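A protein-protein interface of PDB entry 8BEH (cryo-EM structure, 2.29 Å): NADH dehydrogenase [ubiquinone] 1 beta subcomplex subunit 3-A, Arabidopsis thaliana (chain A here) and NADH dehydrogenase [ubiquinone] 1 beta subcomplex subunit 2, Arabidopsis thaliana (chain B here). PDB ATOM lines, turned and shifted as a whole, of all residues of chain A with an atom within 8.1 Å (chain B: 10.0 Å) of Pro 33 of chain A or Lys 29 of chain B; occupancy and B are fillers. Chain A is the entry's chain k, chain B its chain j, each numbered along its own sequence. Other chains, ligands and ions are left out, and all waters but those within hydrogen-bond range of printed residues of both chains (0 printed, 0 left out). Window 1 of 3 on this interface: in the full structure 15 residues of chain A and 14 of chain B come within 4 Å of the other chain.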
ATOM      1  N   MET A  28      -3.700 -29.383 -13.999  1.00  0.00           N
ATOM      2  CA  MET A  28      -3.515 -28.269 -13.074  1.00  0.00           C
ATOM      3  C   MET A  28      -2.777 -28.705 -11.818  1.00  0.00           C
ATOM      4  O   MET A  28      -2.171 -27.873 -11.135  1.00  0.00           O
ATOM      5  CB  MET A  28      -4.862 -27.653 -12.715  1.00  0.00           C
ATOM      6  CG  MET A  28      -5.350 -26.627 -13.723  1.00  0.00           C
ATOM      7  SD  MET A  28      -4.259 -25.199 -13.862  1.00  0.00           S
ATOM      8  CE  MET A  28      -4.724 -24.279 -12.403  1.00  0.00           C
ATOM      9  N   ARG A  29      -2.799 -29.999 -11.505  1.00  0.00           N
ATOM     10  CA  ARG A  29      -2.006 -30.506 -10.397  1.00  0.00           C
ATOM     11  C   ARG A  29      -0.517 -30.559 -10.717  1.00  0.00           C
ATOM     12  O   ARG A  29       0.289 -30.726  -9.796  1.00  0.00           O
ATOM     13  CB  ARG A  29      -2.513 -31.889  -9.983  1.00  0.00           C
ATOM     14  CG  ARG A  29      -3.898 -31.907  -9.373  1.00  0.00           C
ATOM     15  CD  ARG A  29      -4.294 -33.309  -8.951  1.00  0.00           C
ATOM     16  NE  ARG A  29      -5.656 -33.350  -8.426  1.00  0.00           N
ATOM     17  CZ  ARG A  29      -6.304 -34.457  -8.089  1.00  0.00           C
ATOM     18  NH1 ARG A  29      -5.750 -35.652  -8.223  1.00  0.00           N
ATOM     19  NH2 ARG A  29      -7.540 -34.365  -7.607  1.00  0.00           N
ATOM     20  N   HIS A  30      -0.123 -30.416 -11.975  1.00  0.00           N
ATOM     21  CA  HIS A  30       1.293 -30.434 -12.412  1.00  0.00           C
ATOM     22  C   HIS A  30       1.822 -29.042 -12.681  1.00  0.00           C
ATOM     23  O   HIS A  30       2.914 -28.949 -13.192  1.00  0.00           O
ATOM     24  CB  HIS A  30       1.362 -31.231 -13.704  1.00  0.00           C
ATOM     25  CG  HIS A  30       1.431 -32.696 -13.466  1.00  0.00           C
ATOM     26  ND1 HIS A  30       0.308 -33.457 -13.242  1.00  0.00           N
ATOM     27  CD2 HIS A  30       2.486 -33.525 -13.369  1.00  0.00           C
ATOM     28  CE1 HIS A  30       0.666 -34.701 -13.050  1.00  0.00           C
ATOM     29  NE2 HIS A  30       1.994 -34.773 -13.127  1.00  0.00           N
ATOM     30  N   ALA A  31       1.064 -28.015 -12.372  1.00  0.00           N
ATOM     31  CA  ALA A  31       1.377 -26.631 -12.742  1.00  0.00           C
ATOM     32  C   ALA A  31       2.562 -26.010 -11.973  1.00  0.00           C
ATOM     33  O   ALA A  31       3.112 -25.097 -12.471  1.00  0.00           O
ATOM     34  CB  ALA A  31       0.103 -25.895 -12.536  1.00  0.00           C
ATOM     35  N   LEU A  32       2.847 -26.477 -10.748  1.00  0.00           N
ATOM     36  CA  LEU A  32       3.907 -25.911  -9.902  1.00  0.00           C
ATOM     37  C   LEU A  32       4.869 -27.032  -9.528  1.00  0.00           C
ATOM     38  O   LEU A  32       4.905 -27.415  -8.384  1.00  0.00           O
ATOM     39  CB  LEU A  32       3.210 -25.203  -8.725  1.00  0.00           C
ATOM     40  CG  LEU A  32       2.260 -24.062  -9.050  1.00  0.00           C
ATOM     41  CD1 LEU A  32       1.511 -23.654  -7.793  1.00  0.00           C
ATOM     42  CD2 LEU A  32       3.000 -22.884  -9.657  1.00  0.00           C
ATOM     43  N   PRO A  33       5.679 -27.551 -10.474  1.00  0.00           N
ATOM     44  CA  PRO A  33       6.563 -28.670 -10.246  1.00  0.00           C
ATOM     45  C   PRO A  33       7.706 -28.262  -9.327  1.00  0.00           C
ATOM     46  O   PRO A  33       8.147 -27.172  -9.406  1.00  0.00           O
ATOM     47  CB  PRO A  33       7.167 -29.021 -11.627  1.00  0.00           C
ATOM     48  CG  PRO A  33       6.978 -27.793 -12.479  1.00  0.00           C
ATOM     49  CD  PRO A  33       5.838 -27.033 -11.850  1.00  0.00           C
ATOM     50  N   GLY A  34       8.125 -29.210  -8.483  1.00  0.00           N
ATOM     51  CA  GLY A  34       9.099 -28.842  -7.438  1.00  0.00           C
ATOM     52  C   GLY A  34       8.549 -27.929  -6.350  1.00  0.00           C
ATOM     53  O   GLY A  34       9.363 -27.454  -5.597  1.00  0.00           O
ATOM     54  N   ILE A  35       7.276 -27.634  -6.260  1.00  0.00           N
ATOM     55  CA  ILE A  35       6.823 -26.699  -5.187  1.00  0.00           C
ATOM     56  C   ILE A  35       7.053 -27.414  -3.858  1.00  0.00           C
ATOM     57  O   ILE A  35       7.404 -26.758  -2.937  1.00  0.00           O
ATOM     58  CB  ILE A  35       5.372 -26.224  -5.294  1.00  0.00           C
ATOM     59  CG1 ILE A  35       5.057 -25.030  -4.388  1.00  0.00           C
ATOM     60  CG2 ILE A  35       4.396 -27.363  -5.050  1.00  0.00           C
ATOM     61  CD1 ILE A  35       5.631 -23.715  -4.848  1.00  0.00           C
ATOM     62  N   GLY A  36       6.976 -28.737  -3.864  1.00  0.00           N
ATOM     63  CA  GLY A  36       7.184 -29.483  -2.640  1.00  0.00           C
ATOM     64  C   GLY A  36       8.636 -29.570  -2.224  1.00  0.00           C
ATOM     65  O   GLY A  36       8.972 -29.298  -1.067  1.00  0.00           O
ATOM     66  N   ILE A  37       9.505 -29.954  -3.163  1.00  0.00           N
ATOM     67  CA  ILE A  37      10.928 -30.092  -2.861  1.00  0.00           C
ATOM     68  C   ILE A  37      11.522 -28.755  -2.453  1.00  0.00           C
ATOM     69  O   ILE A  37      12.322 -28.677  -1.514  1.00  0.00           O
ATOM     70  CB  ILE A  37      11.679 -30.685  -4.067  1.00  0.00           C
ATOM     71  CG1 ILE A  37      10.950 -31.915  -4.601  1.00  0.00           C
ATOM     72  CG2 ILE A  37      13.107 -31.021  -3.680  1.00  0.00           C
ATOM     73  CD1 ILE A  37      10.794 -31.916  -6.095  1.00  0.00           C
ATOM     74  N   GLY A  38      11.152 -27.683  -3.157  1.00  0.00           N
ATOM     75  CA  GLY A  38      11.679 -26.371  -2.824  1.00  0.00           C
ATOM     76  C   GLY A  38      11.272 -25.914  -1.437  1.00  0.00           C
ATOM     77  O   GLY A  38      12.089 -25.395  -0.676  1.00  0.00           O
ATOM     78  N   PRO B  20       7.526 -39.444 -20.541  1.00  0.00           N
ATOM     79  CA  PRO B  20       8.736 -38.669 -20.822  1.00  0.00           C
ATOM     80  C   PRO B  20       9.987 -39.345 -20.282  1.00  0.00           C
ATOM     81  O   PRO B  20       9.935 -40.214 -19.412  1.00  0.00           O
ATOM     82  CB  PRO B  20       8.475 -37.330 -20.124  1.00  0.00           C
ATOM     83  CG  PRO B  20       7.481 -37.634 -19.070  1.00  0.00           C
ATOM     84  CD  PRO B  20       6.642 -38.776 -19.569  1.00  0.00           C
ATOM     85  N   LYS B  21      11.127 -38.940 -20.836  1.00  0.00           N
ATOM     86  CA  LYS B  21      12.408 -39.437 -20.356  1.00  0.00           C
ATOM     87  C   LYS B  21      12.608 -39.047 -18.899  1.00  0.00           C
ATOM     88  O   LYS B  21      12.234 -37.950 -18.477  1.00  0.00           O
ATOM     89  CB  LYS B  21      13.549 -38.884 -21.208  1.00  0.00           C
ATOM     90  CG  LYS B  21      13.735 -39.586 -22.532  1.00  0.00           C
ATOM     91  CD  LYS B  21      14.790 -38.896 -23.373  1.00  0.00           C
ATOM     92  CE  LYS B  21      15.727 -39.905 -24.018  1.00  0.00           C
ATOM     93  NZ  LYS B  21      15.274 -40.293 -25.382  1.00  0.00           N
ATOM     94  N   THR B  22      13.204 -39.958 -18.127  1.00  0.00           N
ATOM     95  CA  THR B  22      13.301 -39.755 -16.686  1.00  0.00           C
ATOM     96  C   THR B  22      14.114 -38.512 -16.345  1.00  0.00           C
ATOM     97  O   THR B  22      13.714 -37.722 -15.481  1.00  0.00           O
ATOM     98  CB  THR B  22      13.889 -41.002 -16.015  1.00  0.00           C
ATOM     99  OG1 THR B  22      14.065 -40.761 -14.613  1.00  0.00           O
ATOM    100  CG2 THR B  22      15.216 -41.402 -16.645  1.00  0.00           C
ATOM    101  N   TRP B  23      15.229 -38.307 -17.053  1.00  0.00           N
ATOM    102  CA  TRP B  23      16.114 -37.150 -16.751  1.00  0.00           C
ATOM    103  C   TRP B  23      15.402 -35.844 -17.120  1.00  0.00           C
ATOM    104  O   TRP B  23      15.725 -34.820 -16.501  1.00  0.00           O
ATOM    105  CB  TRP B  23      17.479 -37.302 -17.439  1.00  0.00           C
ATOM    106  CG  TRP B  23      17.526 -36.895 -18.879  1.00  0.00           C
ATOM    107  CD1 TRP B  23      17.096 -37.615 -19.956  1.00  0.00           C
ATOM    108  CD2 TRP B  23      18.071 -35.673 -19.405  1.00  0.00           C
ATOM    109  NE1 TRP B  23      17.323 -36.919 -21.113  1.00  0.00           N
ATOM    110  CE2 TRP B  23      17.923 -35.726 -20.808  1.00  0.00           C
ATOM    111  CE3 TRP B  23      18.662 -34.542 -18.832  1.00  0.00           C
ATOM    112  CZ2 TRP B  23      18.342 -34.688 -21.637  1.00  0.00           C
ATOM    113  CZ3 TRP B  23      19.076 -33.517 -19.654  1.00  0.00           C
ATOM    114  CH2 TRP B  23      18.916 -33.590 -21.038  1.00  0.00           C
ATOM    115  N   HIS B  24      14.466 -35.882 -18.076  1.00  0.00           N
ATOM    116  CA  HIS B  24      13.694 -34.689 -18.404  1.00  0.00           C
ATOM    117  C   HIS B  24      12.773 -34.302 -17.253  1.00  0.00           C
ATOM    118  O   HIS B  24      12.741 -33.136 -16.828  1.00  0.00           O
ATOM    119  CB  HIS B  24      12.903 -34.935 -19.685  1.00  0.00           C
ATOM    120  CG  HIS B  24      13.680 -34.642 -20.928  1.00  0.00           C
ATOM    121  ND1 HIS B  24      13.125 -34.692 -22.185  1.00  0.00           N
ATOM    122  CD2 HIS B  24      14.974 -34.292 -21.103  1.00  0.00           C
ATOM    123  CE1 HIS B  24      14.043 -34.387 -23.083  1.00  0.00           C
ATOM    124  NE2 HIS B  24      15.176 -34.141 -22.452  1.00  0.00           N
ATOM    125  N   THR B  25      12.031 -35.277 -16.723  1.00  0.00           N
ATOM    126  CA  THR B  25      11.202 -35.026 -15.552  1.00  0.00           C
ATOM    127  C   THR B  25      12.047 -34.532 -14.389  1.00  0.00           C
ATOM    128  O   THR B  25      11.691 -33.554 -13.725  1.00  0.00           O
ATOM    129  CB  THR B  25      10.440 -36.293 -15.153  1.00  0.00           C
ATOM    130  OG1 THR B  25       9.619 -36.728 -16.242  1.00  0.00           O
ATOM    131  CG2 THR B  25       9.567 -36.027 -13.949  1.00  0.00           C
ATOM    132  N   VAL B  26      13.187 -35.183 -14.147  1.00  0.00           N
ATOM    133  CA  VAL B  26      14.023 -34.827 -13.004  1.00  0.00           C
ATOM    134  C   VAL B  26      14.567 -33.413 -13.156  1.00  0.00           C
ATOM    135  O   VAL B  26      14.555 -32.623 -12.206  1.00  0.00           O
ATOM    136  CB  VAL B  26      15.155 -35.856 -12.823  1.00  0.00           C
ATOM    137  CG1 VAL B  26      16.200 -35.333 -11.848  1.00  0.00           C
ATOM    138  CG2 VAL B  26      14.589 -37.176 -12.337  1.00  0.00           C
ATOM    139  N   THR B  27      15.056 -33.071 -14.351  1.00  0.00           N
ATOM    140  CA  THR B  27      15.611 -31.743 -14.578  1.00  0.00           C
ATOM    141  C   THR B  27      14.550 -30.662 -14.407  1.00  0.00           C
ATOM    142  O   THR B  27      14.812 -29.623 -13.786  1.00  0.00           O
ATOM    143  CB  THR B  27      16.237 -31.680 -15.971  1.00  0.00           C
ATOM    144  OG1 THR B  27      17.357 -32.571 -16.032  1.00  0.00           O
ATOM    145  CG2 THR B  27      16.706 -30.283 -16.290  1.00  0.00           C
ATOM    146  N   GLY B  28      13.345 -30.886 -14.942  1.00  0.00           N
ATOM    147  CA  GLY B  28      12.283 -29.909 -14.752  1.00  0.00           C
ATOM    148  C   GLY B  28      11.900 -29.743 -13.294  1.00  0.00           C
ATOM    149  O   GLY B  28      11.832 -28.619 -12.777  1.00  0.00           O
ATOM    150  N   LYS B  29      11.539 -30.855 -12.621  1.00  0.00           N
ATOM    151  CA  LYS B  29      11.316 -30.754 -11.155  1.00  0.00           C
ATOM    152  C   LYS B  29      12.470 -29.990 -10.472  1.00  0.00           C
ATOM    153  O   LYS B  29      12.118 -28.993  -9.892  1.00  0.00           O
ATOM    154  CB  LYS B  29      11.041 -32.108 -10.496  1.00  0.00           C
ATOM    155  CG  LYS B  29       9.655 -32.685 -10.726  1.00  0.00           C
ATOM    156  CD  LYS B  29       8.665 -32.241  -9.685  1.00  0.00           C
ATOM    157  CE  LYS B  29       7.248 -32.696  -9.957  1.00  0.00           C
ATOM    158  NZ  LYS B  29       6.775 -32.247 -11.286  1.00  0.00           N
ATOM    159  N   GLY B  30      13.746 -30.351 -10.665  1.00  0.00           N
ATOM    160  CA  GLY B  30      14.809 -29.758  -9.877  1.00  0.00           C
ATOM    161  C   GLY B  30      15.026 -28.288 -10.158  1.00  0.00           C
ATOM    162  O   GLY B  30      15.243 -27.505  -9.232  1.00  0.00           O
ATOM    163  N   LEU B  31      14.994 -27.888 -11.433  1.00  0.00           N
ATOM    164  CA  LEU B  31      15.142 -26.472 -11.736  1.00  0.00           C
ATOM    165  C   LEU B  31      13.997 -25.659 -11.156  1.00  0.00           C
ATOM    166  O   LEU B  31      14.223 -24.580 -10.594  1.00  0.00           O
ATOM    167  CB  LEU B  31      15.259 -26.242 -13.241  1.00  0.00           C
ATOM    168  CG  LEU B  31      16.680 -26.345 -13.783  1.00  0.00           C
ATOM    169  CD1 LEU B  31      16.691 -26.964 -15.156  1.00  0.00           C
ATOM    170  CD2 LEU B  31      17.309 -24.965 -13.824  1.00  0.00           C
ATOM    171  N   CYS B  32      12.771 -26.128 -11.276  1.00  0.00           N
ATOM    172  CA  CYS B  32      11.699 -25.374 -10.618  1.00  0.00           C
ATOM    173  C   CYS B  32      11.878 -25.364  -9.084  1.00  0.00           C
ATOM    174  O   CYS B  32      11.565 -24.331  -8.513  1.00  0.00           O
ATOM    175  CB  CYS B  32      10.318 -25.847 -11.086  1.00  0.00           C
ATOM    176  SG  CYS B  32       9.862 -25.156 -12.701  1.00  0.00           S
ATOM    177  N   ALA B  33      12.397 -26.426  -8.482  1.00  0.00           N
ATOM    178  CA  ALA B  33      12.529 -26.494  -7.000  1.00  0.00           C
ATOM    179  C   ALA B  33      13.565 -25.461  -6.610  1.00  0.00           C
ATOM    180  O   ALA B  33      13.268 -24.659  -5.713  1.00  0.00           O
ATOM    181  CB  ALA B  33      12.863 -27.896  -6.531  1.00  0.00           C
ATOM    182  N   VAL B  34      14.603 -25.379  -7.428  1.00  0.00           N
ATOM    183  CA  VAL B  34      15.643 -24.385  -7.195  1.00  0.00           C
ATOM    184  C   VAL B  34      15.062 -22.984  -7.296  1.00  0.00           C
ATOM    185  O   VAL B  34      15.379 -22.108  -6.486  1.00  0.00           O
ATOM    186  CB  VAL B  34      16.809 -24.592  -8.182  1.00  0.00           C
ATOM    187  CG1 VAL B  34      17.568 -23.299  -8.413  1.00  0.00           C
ATOM    188  CG2 VAL B  34      17.746 -25.663  -7.679  1.00  0.00           C
ATOM    189  N   MET B  35      14.193 -22.754  -8.284  1.00  0.00           N
ATOM    190  CA  MET B  35      13.566 -21.443  -8.433  1.00  0.00           C
ATOM    191  C   MET B  35      12.705 -21.089  -7.222  1.00  0.00           C
ATOM    192  O   MET B  35      12.766 -19.963  -6.715  1.00  0.00           O
ATOM    193  CB  MET B  35      12.735 -21.410  -9.715  1.00  0.00           C
ATOM    194  CG  MET B  35      11.696 -20.304  -9.769  1.00  0.00           C
ATOM    195  SD  MET B  35      10.679 -20.364 -11.258  1.00  0.00           S
ATOM    196  CE  MET B  35       9.740 -21.863 -10.965  1.00  0.00           C
ATOM    197  N   TRP B  36      11.898 -21.997  -6.734  1.00  0.00           N
ATOM    198  CA  TRP B  36      11.011 -21.788  -5.545  1.00  0.00           C
ATOM    199  C   TRP B  36      11.860 -21.527  -4.294  1.00  0.00           C
ATOM    200  O   TRP B  36      11.549 -20.572  -3.592  1.00  0.00           O
ATOM    201  CB  TRP B  36      10.027 -22.943  -5.345  1.00  0.00           C
ATOM    202  CG  TRP B  36       9.123 -23.239  -6.501  1.00  0.00           C
ATOM    203  CD1 TRP B  36       8.995 -24.427  -7.154  1.00  0.00           C
ATOM    204  CD2 TRP B  36       8.207 -22.333  -7.136  1.00  0.00           C
ATOM    205  NE1 TRP B  36       8.076 -24.325  -8.156  1.00  0.00           N
ATOM    206  CE2 TRP B  36       7.570 -23.053  -8.169  1.00  0.00           C
ATOM    207  CE3 TRP B  36       7.863 -20.996  -6.944  1.00  0.00           C
ATOM    208  CZ2 TRP B  36       6.604 -22.475  -8.989  1.00  0.00           C
ATOM    209  CZ3 TRP B  36       6.919 -20.417  -7.761  1.00  0.00           C
ATOM    210  CH2 TRP B  36       6.297 -21.153  -8.773  1.00  0.00           C
ATOM    211  N   PHE B  37      12.925 -22.291  -4.121  1.00  0.00           N
ATOM    212  CA  PHE B  37      13.804 -22.064  -2.979  1.00  0.00           C
ATOM    213  C   PHE B  37      14.489 -20.710  -3.073  1.00  0.00           C
ATOM    214  O   PHE B  37      14.623 -20.002  -2.070  1.00  0.00           O
ATOM    215  CB  PHE B  37      14.850 -23.175  -2.881  1.00  0.00           C
ATOM    216  CG  PHE B  37      15.835 -22.981  -1.759  1.00  0.00           C
ATOM    217  CD1 PHE B  37      17.034 -22.319  -1.969  1.00  0.00           C
ATOM    218  CD2 PHE B  37      15.559 -23.463  -0.488  1.00  0.00           C
ATOM    219  CE1 PHE B  37      17.933 -22.139  -0.943  1.00  0.00           C
ATOM    220  CE2 PHE B  37      16.457 -23.287   0.541  1.00  0.00           C
ATOM    221  CZ  PHE B  37      17.646 -22.625   0.314  1.00  0.00           C
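The indole nitrogen of Trp 36 of chain B lies within hydrogen-bond range of the backbone carbonyl oxygen of Pro 33 of chain A (3.1 Å).
Among the printed residues, merely in contact across the chains: Leu 32 of chain A with Trp 36 of chain B (3.7 Å), Pro 33 of chain A with Lys 29 of chain B (3.3 Å), Pro 33 of chain A with Cys 32 of chain B (3.0 Å), Gly 34 of chain A with Lys 29 of chain B (3.3 Å), Gly 34 of chain A with Ala 33 of chain B (3.6 Å), Gly 34 of chain A with Trp 36 of chain B (3.4 Å), Ile 35 of chain A with Trp 36 of chain B (3.7 Å), Ile 37 of chain A with Ala 33 of chain B (3.9 Å), Gly 38 of chain A with Ala 33 of chain B (3.7 Å) and Gly 38 of chain A with Phe 37 of chain B (3.98 Å).
Of the printed residues of chain B, Pro 33 of chain A touches Lys 29 (3.3 Å), Cys 32 (3.0 Å) and Trp 36 (3.1 Å). No residue of chain B comes within 4 Å of Ala 31 of chain A. Of the printed residues of chain B, Gly 34 of chain A touches Lys 29, Ala 33 and Trp 36. No residue of chain A comes within 4 Å of Gly 30 of chain B. Of the printed residues of chain B, Ile 35 of chain A touches Trp 36 (3.7 Å). Of the printed residues of chain B, Ile 37 of chain A touches Ala 33. Of the printed residues of chain A, Ala 33 of chain B touches Gly 34 (3.6 Å), Ile 37 (3.9 Å) and Gly 38 (3.7 Å). Of the printed residues of chain A, Trp 36 of chain B touches Leu 32, Pro 33, Gly 34 and Ile 35. Of the printed residues of chain B, Leu 32 of chain A touches Trp 36. The nearest printed residue of chain A that does not touch Ala 33 of chain B is Pro 33 of chain A (4.4 Å).
Printed residues of chain B that touch a printed residue of chain A: Lys 29, Cys 32, Ala 33, Trp 36 and Phe 37. Hydrophobic or aromatic side chains of chain B that line the printed part of chain A: Ala 33, Trp 36 and Phe 37. Hydrophobic or aromatic side chains of chain A within 4 Å of the printed part of chain B: Leu 32, Pro 33, Ile 35 and Ile 37. Along chain A the printed residues that touch a printed residue of chain B span positions 32 to 38. Among the printed residues, 11 pairs touch across the chains. Among the printed residues, no Asp or Glu carboxylate lies within 4 Å of a Lys or Arg side-chain nitrogen of the other chain.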
